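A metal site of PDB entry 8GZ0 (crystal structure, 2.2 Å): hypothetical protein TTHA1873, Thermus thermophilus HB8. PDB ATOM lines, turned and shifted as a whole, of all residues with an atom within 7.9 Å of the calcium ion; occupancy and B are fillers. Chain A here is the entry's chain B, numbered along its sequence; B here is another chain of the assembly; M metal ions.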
ATOM      1  N   SER A  26      19.676 -18.164  15.686  1.00  0.00           N
ATOM      2  CA  SER A  26      18.636 -18.939  16.358  1.00  0.00           C
ATOM      3  C   SER A  26      17.412 -19.009  15.454  1.00  0.00           C
ATOM      4  O   SER A  26      17.081 -18.006  14.815  1.00  0.00           O
ATOM      5  CB  SER A  26      18.288 -18.333  17.696  1.00  0.00           C
ATOM      6  OG  SER A  26      17.236 -19.060  18.311  1.00  0.00           O
ATOM      7  N   LEU A  27      16.807 -20.204  15.412  1.00  0.00           N
ATOM      8  CA  LEU A  27      15.581 -20.445  14.669  1.00  0.00           C
ATOM      9  C   LEU A  27      14.408 -20.639  15.634  1.00  0.00           C
ATOM     10  O   LEU A  27      13.299 -20.850  15.184  1.00  0.00           O
ATOM     11  CB  LEU A  27      15.737 -21.720  13.827  1.00  0.00           C
ATOM     12  CG  LEU A  27      16.938 -21.794  12.869  1.00  0.00           C
ATOM     13  CD1 LEU A  27      16.768 -22.942  11.879  1.00  0.00           C
ATOM     14  CD2 LEU A  27      17.114 -20.495  12.106  1.00  0.00           C
ATOM     15  N   GLY A  28      14.690 -20.621  16.955  1.00  0.00           N
ATOM     16  CA  GLY A  28      13.684 -20.834  17.976  1.00  0.00           C
ATOM     17  C   GLY A  28      13.412 -22.311  18.225  1.00  0.00           C
ATOM     18  O   GLY A  28      14.195 -23.164  17.773  1.00  0.00           O
ATOM     19  N   GLU A  29      12.284 -22.571  18.909  1.00  0.00           N
ATOM     20  CA  GLU A  29      11.936 -23.889  19.425  1.00  0.00           C
ATOM     21  C   GLU A  29      10.892 -24.555  18.525  1.00  0.00           C
ATOM     22  O   GLU A  29      10.110 -23.892  17.843  1.00  0.00           O
ATOM     23  CB  GLU A  29      11.390 -23.805  20.867  1.00  0.00           C
ATOM     24  CG  GLU A  29      12.364 -23.149  21.852  1.00  0.00           C
ATOM     25  CD  GLU A  29      12.294 -21.641  21.935  1.00  0.00           C
ATOM     26  OE1 GLU A  29      11.632 -21.028  21.073  1.00  0.00           O
ATOM     27  OE2 GLU A  29      12.863 -21.065  22.916  1.00  0.00           O
ATOM     28  N   THR A  39       7.132 -24.222  18.549  1.00  0.00           N
ATOM     29  CA  THR A  39       6.536 -24.112  19.876  1.00  0.00           C
ATOM     30  C   THR A  39       7.208 -22.964  20.641  1.00  0.00           C
ATOM     31  O   THR A  39       7.950 -22.186  20.037  1.00  0.00           O
ATOM     32  CB  THR A  39       6.614 -25.469  20.606  1.00  0.00           C
ATOM     33  OG1 THR A  39       5.767 -25.415  21.760  1.00  0.00           O
ATOM     34  CG2 THR A  39       8.037 -25.822  20.978  1.00  0.00           C
ATOM     35  N   ASP A  40       6.911 -22.888  21.949  1.00  0.00           N
ATOM     36  CA  ASP A  40       7.267 -21.811  22.877  1.00  0.00           C
ATOM     37  C   ASP A  40       6.044 -20.895  23.003  1.00  0.00           C
ATOM     38  O   ASP A  40       5.638 -20.294  22.011  1.00  0.00           O
ATOM     39  CB  ASP A  40       8.517 -21.008  22.483  1.00  0.00           C
ATOM     40  CG  ASP A  40       9.103 -20.183  23.623  1.00  0.00           C
ATOM     41  OD1 ASP A  40       8.610 -20.355  24.808  1.00  0.00           O
ATOM     42  OD2 ASP A  40       9.999 -19.384  23.367  1.00  0.00           O
ATOM     43  N   PRO A  41       5.375 -20.795  24.178  1.00  0.00           N
ATOM     44  CA  PRO A  41       5.782 -21.495  25.405  1.00  0.00           C
ATOM     45  C   PRO A  41       5.680 -23.024  25.348  1.00  0.00           C
ATOM     46  O   PRO A  41       5.112 -23.577  24.421  1.00  0.00           O
ATOM     47  CB  PRO A  41       4.796 -20.973  26.471  1.00  0.00           C
ATOM     48  CG  PRO A  41       4.225 -19.701  25.886  1.00  0.00           C
ATOM     49  CD  PRO A  41       4.174 -19.978  24.401  1.00  0.00           C
ATOM     50  N   VAL A  42       6.292 -23.694  26.344  1.00  0.00           N
ATOM     51  CA  VAL A  42       6.302 -25.137  26.466  1.00  0.00           C
ATOM     52  C   VAL A  42       5.837 -25.490  27.874  1.00  0.00           C
ATOM     53  O   VAL A  42       6.264 -24.850  28.837  1.00  0.00           O
ATOM     54  CB  VAL A  42       7.708 -25.719  26.215  1.00  0.00           C
ATOM     55  CG1 VAL A  42       7.699 -27.242  26.299  1.00  0.00           C
ATOM     56  CG2 VAL A  42       8.300 -25.250  24.897  1.00  0.00           C
ATOM     57  N   TYR A  48      10.964 -30.459  24.064  1.00  0.00           N
ATOM     58  CA  TYR A  48      10.998 -29.525  22.937  1.00  0.00           C
ATOM     59  C   TYR A  48      12.408 -29.491  22.343  1.00  0.00           C
ATOM     60  O   TYR A  48      13.318 -30.110  22.889  1.00  0.00           O
ATOM     61  CB  TYR A  48      10.543 -28.139  23.379  1.00  0.00           C
ATOM     62  CG  TYR A  48      11.473 -27.435  24.333  1.00  0.00           C
ATOM     63  CD1 TYR A  48      11.528 -27.796  25.672  1.00  0.00           C
ATOM     64  CD2 TYR A  48      12.269 -26.394  23.905  1.00  0.00           C
ATOM     65  CE1 TYR A  48      12.352 -27.149  26.572  1.00  0.00           C
ATOM     66  CE2 TYR A  48      13.097 -25.719  24.786  1.00  0.00           C
ATOM     67  CZ  TYR A  48      13.132 -26.094  26.121  1.00  0.00           C
ATOM     68  OH  TYR A  48      13.957 -25.464  27.006  1.00  0.00           O
ATOM     69  N   TYR A  50      15.487 -27.000  20.480  1.00  0.00           N
ATOM     70  CA  TYR A  50      16.128 -25.795  19.983  1.00  0.00           C
ATOM     71  C   TYR A  50      16.752 -26.089  18.620  1.00  0.00           C
ATOM     72  O   TYR A  50      17.258 -27.198  18.406  1.00  0.00           O
ATOM     73  CB  TYR A  50      17.225 -25.336  20.943  1.00  0.00           C
ATOM     74  CG  TYR A  50      16.740 -24.829  22.274  1.00  0.00           C
ATOM     75  CD1 TYR A  50      16.179 -23.557  22.397  1.00  0.00           C
ATOM     76  CD2 TYR A  50      16.909 -25.572  23.431  1.00  0.00           C
ATOM     77  CE1 TYR A  50      15.777 -23.056  23.613  1.00  0.00           C
ATOM     78  CE2 TYR A  50      16.514 -25.080  24.666  1.00  0.00           C
ATOM     79  CZ  TYR A  50      15.946 -23.816  24.756  1.00  0.00           C
ATOM     80  OH  TYR A  50      15.526 -23.320  25.971  1.00  0.00           O
ATOM     81  N   THR A 151      13.685 -20.473  30.508  1.00  0.00           N
ATOM     82  CA  THR A 151      14.961 -21.072  30.175  1.00  0.00           C
ATOM     83  C   THR A 151      15.613 -20.210  29.093  1.00  0.00           C
ATOM     84  O   THR A 151      14.989 -19.975  28.078  1.00  0.00           O
ATOM     85  CB  THR A 151      14.824 -22.532  29.722  1.00  0.00           C
ATOM     86  OG1 THR A 151      14.338 -23.326  30.805  1.00  0.00           O
ATOM     87  CG2 THR A 151      16.141 -23.080  29.247  1.00  0.00           C
ATOM     88  N   PHE A 169      21.515 -15.881  22.079  1.00  0.00           N
ATOM     89  CA  PHE A 169      20.766 -16.293  23.262  1.00  0.00           C
ATOM     90  C   PHE A 169      19.303 -16.459  22.878  1.00  0.00           C
ATOM     91  O   PHE A 169      18.654 -15.499  22.480  1.00  0.00           O
ATOM     92  CB  PHE A 169      20.884 -15.274  24.404  1.00  0.00           C
ATOM     93  CG  PHE A 169      22.291 -15.076  24.927  1.00  0.00           C
ATOM     94  CD1 PHE A 169      23.213 -14.290  24.237  1.00  0.00           C
ATOM     95  CD2 PHE A 169      22.690 -15.705  26.090  1.00  0.00           C
ATOM     96  CE1 PHE A 169      24.514 -14.149  24.706  1.00  0.00           C
ATOM     97  CE2 PHE A 169      23.972 -15.513  26.589  1.00  0.00           C
ATOM     98  CZ  PHE A 169      24.882 -14.764  25.885  1.00  0.00           C
ATOM     99  N   GLU A 170      18.792 -17.693  23.012  1.00  0.00           N
ATOM    100  CA  GLU A 170      17.394 -17.988  22.770  1.00  0.00           C
ATOM    101  C   GLU A 170      16.746 -18.291  24.112  1.00  0.00           C
ATOM    102  O   GLU A 170      17.401 -18.835  25.003  1.00  0.00           O
ATOM    103  CB  GLU A 170      17.267 -19.174  21.784  1.00  0.00           C
ATOM    104  CG  GLU A 170      15.839 -19.558  21.418  1.00  0.00           C
ATOM    105  CD  GLU A 170      15.055 -18.440  20.771  1.00  0.00           C
ATOM    106  OE1 GLU A 170      15.593 -17.837  19.799  1.00  0.00           O
ATOM    107  OE2 GLU A 170      13.949 -18.127  21.276  1.00  0.00           O
ATOM    108  N   THR A 171      15.482 -17.896  24.264  1.00  0.00           N
ATOM    109  CA  THR A 171      14.770 -17.939  25.530  1.00  0.00           C
ATOM    110  C   THR A 171      13.442 -18.671  25.324  1.00  0.00           C
ATOM    111  O   THR A 171      12.733 -18.444  24.343  1.00  0.00           O
ATOM    112  CB  THR A 171      14.587 -16.546  26.170  1.00  0.00           C
ATOM    113  OG1 THR A 171      14.153 -16.635  27.529  1.00  0.00           O
ATOM    114  CG2 THR A 171      13.487 -15.740  25.528  1.00  0.00           C
ATOM    115  N   THR A 172      13.105 -19.542  26.275  1.00  0.00           N
ATOM    116  CA  THR A 172      11.893 -20.357  26.219  1.00  0.00           C
ATOM    117  C   THR A 172      11.059 -20.088  27.473  1.00  0.00           C
ATOM    118  O   THR A 172      11.572 -20.156  28.584  1.00  0.00           O
ATOM    119  CB  THR A 172      12.198 -21.853  26.110  1.00  0.00           C
ATOM    120  OG1 THR A 172      13.265 -22.095  25.179  1.00  0.00           O
ATOM    121  CG2 THR A 172      10.962 -22.665  25.737  1.00  0.00           C
ATOM    122  N   THR A 173       9.770 -19.786  27.269  1.00  0.00           N
ATOM    123  CA  THR A 173       8.791 -19.668  28.336  1.00  0.00           C
ATOM    124  C   THR A 173       8.298 -21.060  28.726  1.00  0.00           C
ATOM    125  O   THR A 173       7.816 -21.808  27.861  1.00  0.00           O
ATOM    126  CB  THR A 173       7.651 -18.734  27.922  1.00  0.00           C
ATOM    127  OG1 THR A 173       8.219 -17.500  27.472  1.00  0.00           O
ATOM    128  CG2 THR A 173       6.657 -18.507  29.040  1.00  0.00           C
ATOM    129  N   ALA B  23       5.762 -15.591  24.807  1.00  0.00           N
ATOM    130  CA  ALA B  23       7.096 -16.052  24.473  1.00  0.00           C
ATOM    131  C   ALA B  23       7.640 -15.231  23.297  1.00  0.00           C
ATOM    132  O   ALA B  23       6.887 -14.638  22.539  1.00  0.00           O
ATOM    133  CB  ALA B  23       7.057 -17.517  24.162  1.00  0.00           C
ATOM    134  N   ILE B  24       8.979 -15.219  23.186  1.00  0.00           N
ATOM    135  CA  ILE B  24       9.695 -14.645  22.046  1.00  0.00           C
ATOM    136  C   ILE B  24      10.696 -15.676  21.493  1.00  0.00           C
ATOM    137  O   ILE B  24      11.193 -16.536  22.232  1.00  0.00           O
ATOM    138  CB  ILE B  24      10.419 -13.348  22.456  1.00  0.00           C
ATOM    139  CG1 ILE B  24      10.933 -12.558  21.240  1.00  0.00           C
ATOM    140  CG2 ILE B  24      11.519 -13.660  23.476  1.00  0.00           C
ATOM    141  CD1 ILE B  24      11.433 -11.158  21.569  1.00  0.00           C
ATOM    142  N   SER B  25      10.959 -15.575  20.190  1.00  0.00           N
ATOM    143  CA  SER B  25      11.955 -16.365  19.504  1.00  0.00           C
ATOM    144  C   SER B  25      12.598 -15.524  18.398  1.00  0.00           C
ATOM    145  O   SER B  25      11.953 -14.663  17.785  1.00  0.00           O
ATOM    146  CB  SER B  25      11.413 -17.681  18.929  1.00  0.00           C
ATOM    147  OG  SER B  25      10.772 -18.488  19.911  1.00  0.00           O
ATOM    148  N   SER B  26      13.895 -15.769  18.174  1.00  0.00           N
ATOM    149  CA  SER B  26      14.578 -15.288  16.984  1.00  0.00           C
ATOM    150  C   SER B  26      14.385 -16.280  15.835  1.00  0.00           C
ATOM    151  O   SER B  26      14.413 -17.468  16.064  1.00  0.00           O
ATOM    152  CB  SER B  26      16.051 -15.039  17.255  1.00  0.00           C
ATOM    153  OG  SER B  26      16.687 -14.532  16.094  1.00  0.00           O
ATOM    154  N   GLU B  53       9.480 -13.589  16.505  1.00  0.00           N
ATOM    155  CA  GLU B  53       8.090 -13.936  16.783  1.00  0.00           C
ATOM    156  C   GLU B  53       7.769 -13.650  18.237  1.00  0.00           C
ATOM    157  O   GLU B  53       8.590 -13.977  19.118  1.00  0.00           O
ATOM    158  CB  GLU B  53       7.794 -15.406  16.496  1.00  0.00           C
ATOM    159  CG  GLU B  53       7.686 -15.714  15.026  1.00  0.00           C
ATOM    160  CD  GLU B  53       7.386 -17.176  14.750  1.00  0.00           C
ATOM    161  OE1 GLU B  53       8.022 -18.035  15.396  1.00  0.00           O
ATOM    162  OE2 GLU B  53       6.508 -17.446  13.873  1.00  0.00           O
ATOM    163  N   ARG B  55       4.669 -14.798  20.762  1.00  0.00           N
ATOM    164  CA  ARG B  55       3.786 -15.966  20.741  1.00  0.00           C
ATOM    165  C   ARG B  55       2.944 -15.973  22.023  1.00  0.00           C
ATOM    166  O   ARG B  55       3.488 -15.949  23.131  1.00  0.00           O
ATOM    167  CB  ARG B  55       4.640 -17.242  20.612  1.00  0.00           C
ATOM    168  CG  ARG B  55       5.769 -17.173  19.572  1.00  0.00           C
ATOM    169  CD  ARG B  55       6.757 -18.304  19.658  1.00  0.00           C
ATOM    170  NE  ARG B  55       6.139 -19.598  19.387  1.00  0.00           N
ATOM    171  CZ  ARG B  55       5.878 -20.119  18.170  1.00  0.00           C
ATOM    172  NH1 ARG B  55       6.350 -19.572  17.074  1.00  0.00           N
ATOM    173  NH2 ARG B  55       5.127 -21.211  18.072  1.00  0.00           N
ATOM    174  N   THR B 167      13.190 -12.083  26.530  1.00  0.00           N
ATOM    175  CA  THR B 167      14.316 -11.467  25.820  1.00  0.00           C
ATOM    176  C   THR B 167      15.185 -12.492  25.096  1.00  0.00           C
ATOM    177  O   THR B 167      15.594 -13.466  25.711  1.00  0.00           O
ATOM    178  CB  THR B 167      15.238 -10.729  26.810  1.00  0.00           C
ATOM    179  OG1 THR B 167      14.440  -9.813  27.555  1.00  0.00           O
ATOM    180  CG2 THR B 167      16.352  -9.971  26.119  1.00  0.00           C
ATOM    181  N   VAL B 168      15.541 -12.203  23.837  1.00  0.00           N
ATOM    182  CA  VAL B 168      16.548 -12.939  23.088  1.00  0.00           C
ATOM    183  C   VAL B 168      17.586 -11.978  22.513  1.00  0.00           C
ATOM    184  O   VAL B 168      17.347 -10.766  22.399  1.00  0.00           O
ATOM    185  CB  VAL B 168      15.919 -13.804  21.974  1.00  0.00           C
ATOM    186  CG1 VAL B 168      15.096 -14.924  22.578  1.00  0.00           C
ATOM    187  CG2 VAL B 168      15.103 -12.976  20.971  1.00  0.00           C
HETATM  188 CA    CA M   1      11.865 -18.809  22.155  1.00  0.00          CA
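The calcium ion is bound by the side-chain carboxylate (OD2) of Asp 40, the side-chain carboxylate (OE2) of Glu 170, the backbone carbonyl oxygen (O) of Ile 24 of chain B, the backbone carbonyl oxygen (O) of Thr 171, the side-chain carboxylate (OE1) of Glu 29, the side-chain hydroxyl (OG) of Ser 25 of chain B and the side-chain carboxylate (OE2) of Glu 29. The calcium ion has seven donor atoms within binding distance.
Within 4 Å of the calcium ion: Glu 29, Asp 40, Glu 170, Thr 171, Ile 24 of chain B and Ser 25 of chain B.
OD1 of Asp 40 is in hydrogen-bond range of N of Thr 173. The guanidinium group (NE) of Arg 55 of chain B is in hydrogen-bond range of the backbone carbonyl oxygen (O) of Asp 40 (2.8 Å). OE1 of Glu 170 is in hydrogen-bond range of N of Ser 26 of chain B. The side-chain carboxylate (OE1) of Glu 170 is in hydrogen-bond range of the side-chain hydroxyl (OG) of Ser 26 of chain A (2.5 Å). The side-chain hydroxyl (OG1) of Thr 171 lies close to the backbone carbonyl oxygen (O) of Thr 151 (3.5 Å). The side-chain hydroxyl of Thr 172 lies close to the side-chain carboxylate of Glu 29, 2.5 Å away. The backbone NH (N) of Thr 39 is in hydrogen-bond range of the backbone carbonyl oxygen (O) of Glu 29. The backbone carbonyl oxygen of Ser 25 of chain B lies within hydrogen-bond range of the backbone NH of Glu 53 of chain B (3.0 Å).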
